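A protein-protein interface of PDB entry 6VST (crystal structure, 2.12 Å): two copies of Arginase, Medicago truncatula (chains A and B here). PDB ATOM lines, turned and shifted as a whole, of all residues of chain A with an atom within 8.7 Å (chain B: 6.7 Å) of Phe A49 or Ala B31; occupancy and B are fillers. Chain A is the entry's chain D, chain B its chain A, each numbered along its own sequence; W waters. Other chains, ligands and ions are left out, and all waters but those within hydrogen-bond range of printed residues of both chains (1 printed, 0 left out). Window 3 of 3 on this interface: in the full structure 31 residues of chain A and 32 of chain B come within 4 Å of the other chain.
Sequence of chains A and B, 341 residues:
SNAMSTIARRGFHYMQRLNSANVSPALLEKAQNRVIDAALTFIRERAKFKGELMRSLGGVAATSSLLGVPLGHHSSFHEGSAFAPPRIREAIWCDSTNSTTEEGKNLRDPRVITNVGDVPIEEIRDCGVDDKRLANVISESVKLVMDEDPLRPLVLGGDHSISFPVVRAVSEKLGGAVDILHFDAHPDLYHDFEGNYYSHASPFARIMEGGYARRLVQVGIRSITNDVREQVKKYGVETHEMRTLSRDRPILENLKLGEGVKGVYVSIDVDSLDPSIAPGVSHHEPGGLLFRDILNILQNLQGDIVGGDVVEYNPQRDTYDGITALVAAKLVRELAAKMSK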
ATOM      1  N   PHE A  42     -28.419  -6.383   8.125  1.00  0.00           N
ATOM      2  CA  PHE A  42     -27.883  -7.542   7.420  1.00  0.00           C
ATOM      3  C   PHE A  42     -26.913  -8.323   8.303  1.00  0.00           C
ATOM      4  O   PHE A  42     -27.007  -9.550   8.418  1.00  0.00           O
ATOM      5  CB  PHE A  42     -27.200  -7.116   6.124  1.00  0.00           C
ATOM      6  CG  PHE A  42     -26.836  -8.271   5.250  1.00  0.00           C
ATOM      7  CD1 PHE A  42     -27.830  -9.054   4.673  1.00  0.00           C
ATOM      8  CD2 PHE A  42     -25.514  -8.602   5.035  1.00  0.00           C
ATOM      9  CE1 PHE A  42     -27.509 -10.134   3.879  1.00  0.00           C
ATOM     10  CE2 PHE A  42     -25.176  -9.683   4.232  1.00  0.00           C
ATOM     11  CZ  PHE A  42     -26.173 -10.453   3.653  1.00  0.00           C
ATOM     12  N   ILE A  43     -25.969  -7.626   8.931  1.00  0.00           N
ATOM     13  CA  ILE A  43     -25.036  -8.285   9.840  1.00  0.00           C
ATOM     14  C   ILE A  43     -25.788  -8.951  10.991  1.00  0.00           C
ATOM     15  O   ILE A  43     -25.470 -10.083  11.382  1.00  0.00           O
ATOM     16  CB  ILE A  43     -23.983  -7.273  10.346  1.00  0.00           C
ATOM     17  CG1 ILE A  43     -23.147  -6.729   9.184  1.00  0.00           C
ATOM     18  CG2 ILE A  43     -23.085  -7.880  11.433  1.00  0.00           C
ATOM     19  CD1 ILE A  43     -22.485  -7.799   8.355  1.00  0.00           C
ATOM     20  N   ARG A  44     -26.799  -8.266  11.549  1.00  0.00           N
ATOM     21  CA  ARG A  44     -27.562  -8.846  12.654  1.00  0.00           C
ATOM     22  C   ARG A  44     -28.192 -10.170  12.240  1.00  0.00           C
ATOM     23  O   ARG A  44     -28.068 -11.176  12.948  1.00  0.00           O
ATOM     24  CB  ARG A  44     -28.644  -7.874  13.157  1.00  0.00           C
ATOM     25  CG  ARG A  44     -29.272  -8.294  14.486  1.00  0.00           C
ATOM     26  CD  ARG A  44     -30.509  -7.451  14.885  1.00  0.00           C
ATOM     27  NE  ARG A  44     -30.495  -6.161  14.206  1.00  0.00           N
ATOM     28  CZ  ARG A  44     -30.086  -5.019  14.751  1.00  0.00           C
ATOM     29  NH1 ARG A  44     -29.690  -4.983  16.024  1.00  0.00           N
ATOM     30  NH2 ARG A  44     -30.089  -3.903  14.021  1.00  0.00           N
ATOM     31  N   GLU A  45     -28.859 -10.193  11.080  1.00  0.00           N
ATOM     32  CA  GLU A  45     -29.546 -11.416  10.668  1.00  0.00           C
ATOM     33  C   GLU A  45     -28.551 -12.532  10.370  1.00  0.00           C
ATOM     34  O   GLU A  45     -28.799 -13.697  10.712  1.00  0.00           O
ATOM     35  CB  GLU A  45     -30.450 -11.162   9.452  1.00  0.00           C
ATOM     36  CG  GLU A  45     -31.581 -10.143   9.655  1.00  0.00           C
ATOM     37  CD  GLU A  45     -32.684 -10.621  10.580  1.00  0.00           C
ATOM     38  OE1 GLU A  45     -32.586 -11.755  11.103  1.00  0.00           O
ATOM     39  OE2 GLU A  45     -33.663  -9.858  10.775  1.00  0.00           O
ATOM     40  N   ARG A  46     -27.419 -12.197   9.744  1.00  0.00           N
ATOM     41  CA  ARG A  46     -26.384 -13.197   9.497  1.00  0.00           C
ATOM     42  C   ARG A  46     -25.832 -13.744  10.808  1.00  0.00           C
ATOM     43  O   ARG A  46     -25.697 -14.963  10.977  1.00  0.00           O
ATOM     44  CB  ARG A  46     -25.264 -12.595   8.644  1.00  0.00           C
ATOM     45  CG  ARG A  46     -25.642 -12.417   7.173  1.00  0.00           C
ATOM     46  CD  ARG A  46     -25.556 -13.731   6.420  1.00  0.00           C
ATOM     47  NE  ARG A  46     -24.167 -14.179   6.336  1.00  0.00           N
ATOM     48  CZ  ARG A  46     -23.789 -15.404   5.985  1.00  0.00           C
ATOM     49  NH1 ARG A  46     -24.697 -16.318   5.687  1.00  0.00           N
ATOM     50  NH2 ARG A  46     -22.499 -15.711   5.938  1.00  0.00           N
ATOM     51  N   ALA A  47     -25.522 -12.855  11.755  1.00  0.00           N
ATOM     52  CA  ALA A  47     -25.047 -13.302  13.059  1.00  0.00           C
ATOM     53  C   ALA A  47     -26.085 -14.173  13.757  1.00  0.00           C
ATOM     54  O   ALA A  47     -25.736 -15.182  14.378  1.00  0.00           O
ATOM     55  CB  ALA A  47     -24.684 -12.098  13.926  1.00  0.00           C
ATOM     56  N   LYS A  48     -27.366 -13.797  13.665  1.00  0.00           N
ATOM     57  CA  LYS A  48     -28.438 -14.584  14.274  1.00  0.00           C
ATOM     58  C   LYS A  48     -28.555 -15.959  13.621  1.00  0.00           C
ATOM     59  O   LYS A  48     -28.773 -16.967  14.305  1.00  0.00           O
ATOM     60  CB  LYS A  48     -29.758 -13.820  14.162  1.00  0.00           C
ATOM     61  CG  LYS A  48     -31.010 -14.570  14.612  1.00  0.00           C
ATOM     62  CD  LYS A  48     -32.169 -13.593  14.761  1.00  0.00           C
ATOM     63  CE  LYS A  48     -33.446 -14.111  14.133  1.00  0.00           C
ATOM     64  NZ  LYS A  48     -34.068 -15.180  14.957  1.00  0.00           N
ATOM     65  N   PHE A  49     -28.425 -16.008  12.295  1.00  0.00           N
ATOM     66  CA  PHE A  49     -28.408 -17.274  11.565  1.00  0.00           C
ATOM     67  C   PHE A  49     -27.305 -18.188  12.085  1.00  0.00           C
ATOM     68  O   PHE A  49     -27.554 -19.339  12.462  1.00  0.00           O
ATOM     69  CB  PHE A  49     -28.216 -16.977  10.073  1.00  0.00           C
ATOM     70  CG  PHE A  49     -28.358 -18.168   9.170  1.00  0.00           C
ATOM     71  CD1 PHE A  49     -27.324 -19.072   9.016  1.00  0.00           C
ATOM     72  CD2 PHE A  49     -29.513 -18.353   8.426  1.00  0.00           C
ATOM     73  CE1 PHE A  49     -27.449 -20.165   8.164  1.00  0.00           C
ATOM     74  CE2 PHE A  49     -29.644 -19.446   7.571  1.00  0.00           C
ATOM     75  CZ  PHE A  49     -28.605 -20.350   7.440  1.00  0.00           C
ATOM     76  N   LYS A  50     -26.070 -17.685  12.110  1.00  0.00           N
ATOM     77  CA  LYS A  50     -24.945 -18.503  12.547  1.00  0.00           C
ATOM     78  C   LYS A  50     -25.030 -18.829  14.038  1.00  0.00           C
ATOM     79  O   LYS A  50     -24.748 -19.963  14.446  1.00  0.00           O
ATOM     80  CB  LYS A  50     -23.636 -17.790  12.201  1.00  0.00           C
ATOM     81  CG  LYS A  50     -23.422 -17.676  10.700  1.00  0.00           C
ATOM     82  CD  LYS A  50     -23.570 -19.051  10.057  1.00  0.00           C
ATOM     83  CE  LYS A  50     -23.528 -18.990   8.543  1.00  0.00           C
ATOM     84  NZ  LYS A  50     -22.128 -18.861   8.034  1.00  0.00           N
ATOM     85  N   GLY A  51     -25.408 -17.859  14.870  1.00  0.00           N
ATOM     86  CA  GLY A  51     -25.526 -18.133  16.295  1.00  0.00           C
ATOM     87  C   GLY A  51     -26.553 -19.212  16.601  1.00  0.00           C
ATOM     88  O   GLY A  51     -26.304 -20.121  17.397  1.00  0.00           O
ATOM     89  N   GLU A  52     -27.724 -19.128  15.963  1.00  0.00           N
ATOM     90  CA  GLU A  52     -28.730 -20.170  16.137  1.00  0.00           C
ATOM     91  C   GLU A  52     -28.198 -21.534  15.708  1.00  0.00           C
ATOM     92  O   GLU A  52     -28.381 -22.533  16.413  1.00  0.00           O
ATOM     93  CB  GLU A  52     -29.992 -19.805  15.362  1.00  0.00           C
ATOM     94  CG  GLU A  52     -30.947 -18.924  16.167  1.00  0.00           C
ATOM     95  CD  GLU A  52     -32.040 -18.305  15.318  1.00  0.00           C
ATOM     96  OE1 GLU A  52     -32.068 -18.562  14.093  1.00  0.00           O
ATOM     97  OE2 GLU A  52     -32.861 -17.550  15.873  1.00  0.00           O
ATOM     98  N   LEU A  53     -27.526 -21.591  14.556  1.00  0.00           N
ATOM     99  CA  LEU A  53     -26.969 -22.851  14.078  1.00  0.00           C
ATOM    100  C   LEU A  53     -26.022 -23.470  15.105  1.00  0.00           C
ATOM    101  O   LEU A  53     -26.115 -24.667  15.401  1.00  0.00           O
ATOM    102  CB  LEU A  53     -26.250 -22.632  12.745  1.00  0.00           C
ATOM    103  CG  LEU A  53     -25.350 -23.781  12.282  1.00  0.00           C
ATOM    104  CD1 LEU A  53     -26.196 -25.000  11.952  1.00  0.00           C
ATOM    105  CD2 LEU A  53     -24.502 -23.373  11.092  1.00  0.00           C
ATOM    106  N   MET A  54     -25.100 -22.668  15.660  1.00  0.00           N
ATOM    107  CA  MET A  54     -24.151 -23.191  16.645  1.00  0.00           C
ATOM    108  C   MET A  54     -24.867 -23.669  17.900  1.00  0.00           C
ATOM    109  O   MET A  54     -24.499 -24.694  18.479  1.00  0.00           O
ATOM    110  CB  MET A  54     -23.106 -22.141  17.037  1.00  0.00           C
ATOM    111  CG  MET A  54     -22.384 -21.488  15.894  1.00  0.00           C
ATOM    112  SD  MET A  54     -21.661 -22.659  14.738  1.00  0.00           S
ATOM    113  CE  MET A  54     -21.843 -21.723  13.225  1.00  0.00           C
ATOM    114  N   ARG A  55     -25.877 -22.927  18.351  1.00  0.00           N
ATOM    115  CA  ARG A  55     -26.592 -23.342  19.550  1.00  0.00           C
ATOM    116  C   ARG A  55     -27.320 -24.665  19.328  1.00  0.00           C
ATOM    117  O   ARG A  55     -27.353 -25.511  20.225  1.00  0.00           O
ATOM    118  CB  ARG A  55     -27.542 -22.229  20.002  1.00  0.00           C
ATOM    119  CG  ARG A  55     -26.778 -20.986  20.460  1.00  0.00           C
ATOM    120  CD  ARG A  55     -27.593 -20.027  21.295  1.00  0.00           C
ATOM    121  NE  ARG A  55     -28.631 -19.333  20.538  1.00  0.00           N
ATOM    122  CZ  ARG A  55     -28.426 -18.263  19.779  1.00  0.00           C
ATOM    123  NH1 ARG A  55     -27.203 -17.753  19.645  1.00  0.00           N
ATOM    124  NH2 ARG A  55     -29.448 -17.707  19.142  1.00  0.00           N
ATOM    125  N   SER A  56     -27.860 -24.888  18.127  1.00  0.00           N
ATOM    126  CA  SER A  56     -28.536 -26.150  17.838  1.00  0.00           C
ATOM    127  C   SER A  56     -27.567 -27.315  17.672  1.00  0.00           C
ATOM    128  O   SER A  56     -27.988 -28.470  17.754  1.00  0.00           O
ATOM    129  CB  SER A  56     -29.380 -26.022  16.574  1.00  0.00           C
ATOM    130  OG  SER A  56     -28.562 -26.199  15.428  1.00  0.00           O
ATOM    131  N   THR A 114     -16.800 -19.821  10.973  1.00  0.00           N
ATOM    132  CA  THR A 114     -18.005 -19.527  10.217  1.00  0.00           C
ATOM    133  C   THR A 114     -17.896 -18.115   9.661  1.00  0.00           C
ATOM    134  O   THR A 114     -17.134 -17.294  10.162  1.00  0.00           O
ATOM    135  CB  THR A 114     -19.280 -19.724  11.076  1.00  0.00           C
ATOM    136  OG1 THR A 114     -20.399 -19.917  10.210  1.00  0.00           O
ATOM    137  CG2 THR A 114     -19.564 -18.534  12.003  1.00  0.00           C
ATOM    138  N   ASN A 115     -18.653 -17.847   8.601  1.00  0.00           N
ATOM    139  CA  ASN A 115     -18.668 -16.535   7.968  1.00  0.00           C
ATOM    140  C   ASN A 115     -19.895 -15.736   8.411  1.00  0.00           C
ATOM    141  O   ASN A 115     -21.016 -16.251   8.409  1.00  0.00           O
ATOM    142  CB  ASN A 115     -18.638 -16.667   6.442  1.00  0.00           C
ATOM    143  CG  ASN A 115     -18.464 -15.323   5.744  1.00  0.00           C
ATOM    144  OD1 ASN A 115     -17.765 -14.429   6.248  1.00  0.00           O
ATOM    145  ND2 ASN A 115     -19.113 -15.162   4.591  1.00  0.00           N
ATOM    146  N   VAL A 116     -19.685 -14.485   8.801  1.00  0.00           N
ATOM    147  CA  VAL A 116     -20.793 -13.574   9.086  1.00  0.00           C
ATOM    148  C   VAL A 116     -21.089 -12.671   7.892  1.00  0.00           C
ATOM    149  O   VAL A 116     -22.216 -12.622   7.404  1.00  0.00           O
ATOM    150  CB  VAL A 116     -20.515 -12.752  10.363  1.00  0.00           C
ATOM    151  CG1 VAL A 116     -21.565 -11.679  10.526  1.00  0.00           C
ATOM    152  CG2 VAL A 116     -20.507 -13.646  11.573  1.00  0.00           C
ATOM    153  N   GLU A 148     -24.343 -12.684  19.716  1.00  0.00           N
ATOM    154  CA  GLU A 148     -24.822 -14.036  19.430  1.00  0.00           C
ATOM    155  C   GLU A 148     -23.856 -15.052  20.027  1.00  0.00           C
ATOM    156  O   GLU A 148     -22.829 -15.384  19.426  1.00  0.00           O
ATOM    157  CB  GLU A 148     -24.977 -14.246  17.925  1.00  0.00           C
ATOM    158  CG  GLU A 148     -26.092 -13.424  17.295  1.00  0.00           C
ATOM    159  CD  GLU A 148     -27.477 -13.868  17.725  1.00  0.00           C
ATOM    160  OE1 GLU A 148     -27.616 -14.947  18.349  1.00  0.00           O
ATOM    161  OE2 GLU A 148     -28.441 -13.136  17.427  1.00  0.00           O
ATOM    162  N   ASP A 149     -24.185 -15.535  21.219  1.00  0.00           N
ATOM    163  CA  ASP A 149     -23.504 -16.681  21.796  1.00  0.00           C
ATOM    164  C   ASP A 149     -23.521 -17.848  20.807  1.00  0.00           C
ATOM    165  O   ASP A 149     -24.590 -18.186  20.280  1.00  0.00           O
ATOM    166  CB  ASP A 149     -24.201 -17.082  23.097  1.00  0.00           C
ATOM    167  CG  ASP A 149     -23.480 -18.188  23.822  1.00  0.00           C
ATOM    168  OD1 ASP A 149     -22.286 -18.010  24.129  1.00  0.00           O
ATOM    169  OD2 ASP A 149     -24.107 -19.228  24.101  1.00  0.00           O
ATOM    170  N   LEU A 151     -20.556 -16.838  19.186  1.00  0.00           N
ATOM    171  CA  LEU A 151     -19.699 -16.256  18.165  1.00  0.00           C
ATOM    172  C   LEU A 151     -18.695 -15.298  18.793  1.00  0.00           C
ATOM    173  O   LEU A 151     -19.017 -14.573  19.737  1.00  0.00           O
ATOM    174  CB  LEU A 151     -20.540 -15.514  17.124  1.00  0.00           C
ATOM    175  CG  LEU A 151     -21.703 -16.269  16.469  1.00  0.00           C
ATOM    176  CD1 LEU A 151     -22.172 -15.522  15.212  1.00  0.00           C
ATOM    177  CD2 LEU A 151     -21.279 -17.698  16.131  1.00  0.00           C
ATOM    178  N   ALA B  26     -38.580 -26.767   7.281  1.00  0.00           N
ATOM    179  CA  ALA B  26     -39.373 -25.568   7.031  1.00  0.00           C
ATOM    180  C   ALA B  26     -38.831 -24.377   7.811  1.00  0.00           C
ATOM    181  O   ALA B  26     -39.025 -23.227   7.400  1.00  0.00           O
ATOM    182  CB  ALA B  26     -40.839 -25.820   7.386  1.00  0.00           C
ATOM    183  N   LEU B  27     -38.152 -24.637   8.934  1.00  0.00           N
ATOM    184  CA  LEU B  27     -37.508 -23.571   9.697  1.00  0.00           C
ATOM    185  C   LEU B  27     -36.299 -23.014   8.952  1.00  0.00           C
ATOM    186  O   LEU B  27     -36.027 -21.807   9.003  1.00  0.00           O
ATOM    187  CB  LEU B  27     -37.098 -24.101  11.075  1.00  0.00           C
ATOM    188  CG  LEU B  27     -36.550 -23.176  12.172  1.00  0.00           C
ATOM    189  CD1 LEU B  27     -36.723 -23.836  13.535  1.00  0.00           C
ATOM    190  CD2 LEU B  27     -35.080 -22.804  11.953  1.00  0.00           C
ATOM    191  N   LEU B  28     -35.558 -23.880   8.263  1.00  0.00           N
ATOM    192  CA  LEU B  28     -34.365 -23.429   7.559  1.00  0.00           C
ATOM    193  C   LEU B  28     -34.715 -22.400   6.495  1.00  0.00           C
ATOM    194  O   LEU B  28     -33.988 -21.418   6.308  1.00  0.00           O
ATOM    195  CB  LEU B  28     -33.648 -24.628   6.940  1.00  0.00           C
ATOM    196  CG  LEU B  28     -33.016 -25.741   7.788  1.00  0.00           C
ATOM    197  CD1 LEU B  28     -32.511 -26.862   6.893  1.00  0.00           C
ATOM    198  CD2 LEU B  28     -31.908 -25.253   8.718  1.00  0.00           C
ATOM    199  N   GLU B  29     -35.834 -22.596   5.794  1.00  0.00           N
ATOM    200  CA  GLU B  29     -36.142 -21.689   4.697  1.00  0.00           C
ATOM    201  C   GLU B  29     -36.578 -20.326   5.210  1.00  0.00           C
ATOM    202  O   GLU B  29     -36.325 -19.309   4.553  1.00  0.00           O
ATOM    203  CB  GLU B  29     -37.205 -22.292   3.781  1.00  0.00           C
ATOM    204  CG  GLU B  29     -36.932 -21.992   2.304  1.00  0.00           C
ATOM    205  CD  GLU B  29     -37.780 -22.818   1.352  1.00  0.00           C
ATOM    206  OE1 GLU B  29     -38.838 -23.332   1.789  1.00  0.00           O
ATOM    207  OE2 GLU B  29     -37.379 -22.955   0.169  1.00  0.00           O
ATOM    208  N   LYS B  30     -37.213 -20.279   6.381  1.00  0.00           N
ATOM    209  CA  LYS B  30     -37.571 -18.990   6.961  1.00  0.00           C
ATOM    210  C   LYS B  30     -36.331 -18.213   7.373  1.00  0.00           C
ATOM    211  O   LYS B  30     -36.297 -16.984   7.258  1.00  0.00           O
ATOM    212  CB  LYS B  30     -38.500 -19.181   8.158  1.00  0.00           C
ATOM    213  CG  LYS B  30     -39.971 -19.248   7.787  1.00  0.00           C
ATOM    214  CD  LYS B  30     -40.862 -19.217   9.022  1.00  0.00           C
ATOM    215  CE  LYS B  30     -40.701 -17.910   9.789  1.00  0.00           C
ATOM    216  NZ  LYS B  30     -41.599 -17.840  10.978  1.00  0.00           N
ATOM    217  N   ALA B  31     -35.301 -18.913   7.847  1.00  0.00           N
ATOM    218  CA  ALA B  31     -34.075 -18.236   8.248  1.00  0.00           C
ATOM    219  C   ALA B  31     -33.330 -17.677   7.035  1.00  0.00           C
ATOM    220  O   ALA B  31     -32.863 -16.531   7.060  1.00  0.00           O
ATOM    221  CB  ALA B  31     -33.197 -19.195   9.048  1.00  0.00           C
ATOM    222  N   GLN B  32     -33.206 -18.471   5.961  1.00  0.00           N
ATOM    223  CA  GLN B  32     -32.635 -17.952   4.715  1.00  0.00           C
ATOM    224  C   GLN B  32     -33.425 -16.753   4.211  1.00  0.00           C
ATOM    225  O   GLN B  32     -32.849 -15.784   3.703  1.00  0.00           O
ATOM    226  CB  GLN B  32     -32.619 -19.032   3.626  1.00  0.00           C
ATOM    227  CG  GLN B  32     -31.771 -20.251   3.921  1.00  0.00           C
ATOM    228  CD  GLN B  32     -32.165 -21.453   3.067  1.00  0.00           C
ATOM    229  OE1 GLN B  32     -33.307 -21.561   2.620  1.00  0.00           O
ATOM    230  NE2 GLN B  32     -31.220 -22.355   2.838  1.00  0.00           N
ATOM    231  N   ASN B  33     -34.752 -16.811   4.336  1.00  0.00           N
ATOM    232  CA  ASN B  33     -35.595 -15.742   3.827  1.00  0.00           C
ATOM    233  C   ASN B  33     -35.355 -14.432   4.563  1.00  0.00           C
ATOM    234  O   ASN B  33     -35.460 -13.363   3.955  1.00  0.00           O
ATOM    235  CB  ASN B  33     -37.067 -16.160   3.918  1.00  0.00           C
ATOM    236  CG  ASN B  33     -37.486 -17.035   2.742  1.00  0.00           C
ATOM    237  OD1 ASN B  33     -36.645 -17.460   1.939  1.00  0.00           O
ATOM    238  ND2 ASN B  33     -38.782 -17.286   2.619  1.00  0.00           N
ATOM    239  N   ARG B  34     -35.032 -14.491   5.858  1.00  0.00           N
ATOM    240  CA  ARG B  34     -34.710 -13.269   6.592  1.00  0.00           C
ATOM    241  C   ARG B  34     -33.391 -12.665   6.106  1.00  0.00           C
ATOM    242  O   ARG B  34     -33.269 -11.439   5.985  1.00  0.00           O
ATOM    243  CB  ARG B  34     -34.656 -13.558   8.088  1.00  0.00           C
ATOM    244  CG  ARG B  34     -35.973 -14.071   8.674  1.00  0.00           C
ATOM    245  CD  ARG B  34     -35.851 -14.273  10.178  1.00  0.00           C
ATOM    246  NE  ARG B  34     -35.451 -13.021  10.806  1.00  0.00           N
ATOM    247  CZ  ARG B  34     -36.257 -12.243  11.521  1.00  0.00           C
ATOM    248  NH1 ARG B  34     -35.790 -11.110  12.035  1.00  0.00           N
ATOM    249  NH2 ARG B  34     -37.519 -12.604  11.743  1.00  0.00           N
ATOM    250  N   VAL B  35     -32.398 -13.508   5.804  1.00  0.00           N
ATOM    251  CA  VAL B  35     -31.142 -13.004   5.243  1.00  0.00           C
ATOM    252  C   VAL B  35     -31.393 -12.365   3.886  1.00  0.00           C
ATOM    253  O   VAL B  35     -30.920 -11.257   3.605  1.00  0.00           O
ATOM    254  CB  VAL B  35     -30.089 -14.127   5.157  1.00  0.00           C
ATOM    255  CG1 VAL B  35     -28.872 -13.663   4.383  1.00  0.00           C
ATOM    256  CG2 VAL B  35     -29.669 -14.585   6.555  1.00  0.00           C
ATOM    257  N   ILE B  36     -32.161 -13.045   3.030  1.00  0.00           N
ATOM    258  CA  ILE B  36     -32.399 -12.542   1.678  1.00  0.00           C
ATOM    259  C   ILE B  36     -33.152 -11.216   1.723  1.00  0.00           C
ATOM    260  O   ILE B  36     -32.787 -10.256   1.035  1.00  0.00           O
ATOM    261  CB  ILE B  36     -33.151 -13.590   0.841  1.00  0.00           C
ATOM    262  CG1 ILE B  36     -32.169 -14.620   0.289  1.00  0.00           C
ATOM    263  CG2 ILE B  36     -33.920 -12.925  -0.292  1.00  0.00           C
ATOM    264  CD1 ILE B  36     -32.821 -15.921  -0.120  1.00  0.00           C
ATOM    265  N   ASP B 126     -23.833 -18.880   1.294  1.00  0.00           N
ATOM    266  CA  ASP B 126     -23.430 -19.428   2.581  1.00  0.00           C
ATOM    267  C   ASP B 126     -24.610 -19.736   3.493  1.00  0.00           C
ATOM    268  O   ASP B 126     -24.401 -20.302   4.571  1.00  0.00           O
ATOM    269  CB  ASP B 126     -22.472 -18.433   3.258  1.00  0.00           C
ATOM    270  CG  ASP B 126     -21.797 -19.002   4.490  1.00  0.00           C
ATOM    271  OD1 ASP B 126     -20.924 -19.879   4.345  1.00  0.00           O
ATOM    272  OD2 ASP B 126     -22.129 -18.569   5.612  1.00  0.00           O
ATOM    273  N   CYS B 127     -25.835 -19.370   3.113  1.00  0.00           N
ATOM    274  CA  CYS B 127     -27.020 -19.759   3.875  1.00  0.00           C
ATOM    275  C   CYS B 127     -27.639 -21.054   3.374  1.00  0.00           C
ATOM    276  O   CYS B 127     -28.678 -21.469   3.897  1.00  0.00           O
ATOM    277  CB  CYS B 127     -28.081 -18.649   3.838  1.00  0.00           C
ATOM    278  SG  CYS B 127     -27.632 -17.160   4.744  1.00  0.00           S
ATOM    279  N   GLY B 128     -27.035 -21.692   2.376  1.00  0.00           N
ATOM    280  CA  GLY B 128     -27.596 -22.890   1.789  1.00  0.00           C
ATOM    281  C   GLY B 128     -28.635 -22.644   0.725  1.00  0.00           C
ATOM    282  O   GLY B 128     -29.325 -23.582   0.326  1.00  0.00           O
HETATM  283  O   HOH W   1     -19.549 -19.960   6.942  1.00  0.00           O
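The guanidinium group (NH1) of Arg B34 is in salt-bridge range of the side-chain carboxylate (OE2) of Glu A45, at 2.8 Å. The side-chain carboxylate (OD2) of Asp B126 is in salt-bridge range of the guanidinium group (NH2) of Arg A46 (2.9 Å). OD2 of Asp B126 is in salt-bridge range of NZ of Lys A50, 2.4 Å away. SG of Cys B127 lies within hydrogen-bond range of NH1 of Arg A46 (3.2 Å).
NE2 of Gln B32 sits at hydrogen-bond distance from O of Cys B127. NH2 of Arg A46 is in hydrogen-bond range of O of Asn A115 (2.9 Å). The guanidinium group (NE) of Arg A46 lies within hydrogen-bond range of the backbone carbonyl oxygen (O) of Val A116. The side-chain hydroxyl of Thr A114 sits at hydrogen-bond distance from the side-chain amino group of Lys A50. The backbone carbonyl oxygen (O) of Asn A115 sits at hydrogen-bond distance from the side-chain amino group (NZ) of Lys A50.
CE1 of Phe A42 touches O of Val B35 (3.6 Å). CD of Arg A46 touches CG1 of Val B35 (3.9 Å). CD2 of Phe A49 touches CB of Ala B31, at 3.8 Å. Cys B127 touches Phe A49. Asp B126 touches Asn A115.
Of chain B, only Ala B31 and Cys B127 come within 4 Å of Phe A49. Printed residues of chain B within 4 Å of Glu A45: Arg B34 (2.8 Å). Printed residues of chain B within 4 Å of Phe A42: Val B35 (3.6 Å). Of the printed residues of chain A, Cys B127 touches Arg A46 (3.2 Å) and Phe A49 (3.7 Å). Of the printed residues of chain A, Val B35 touches Phe A42 and Arg A46. Of the printed residues of chain A, Asp B126 touches Arg A46, Lys A50 and Asn A115. The nearest residue of chain B that does not touch Phe A49 is Gln B32 (4.03 Å). The nearest residue of chain A that does not touch Ala B31 is Glu A52 (5.2 Å). The nearest printed residue of chain A that does not touch Cys B127 is Lys A50 (5.9 Å).
Along chain A the printed residues that touch a printed residue of chain B span positions 42 to 115. Of the 14 printed residues of chain B, 5 touch a printed residue of chain A. Among the printed residues, 9 pairs touch across the chains.
No position is printed for both chains.
Water W1 lies within hydrogen-bond range of N of Asn A115 (2.8 Å), OD1 of Asp B126 (2.9 Å), NZ of Lys A50 (3.0 Å) and OG1 of Thr A114 (3.4 Å).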
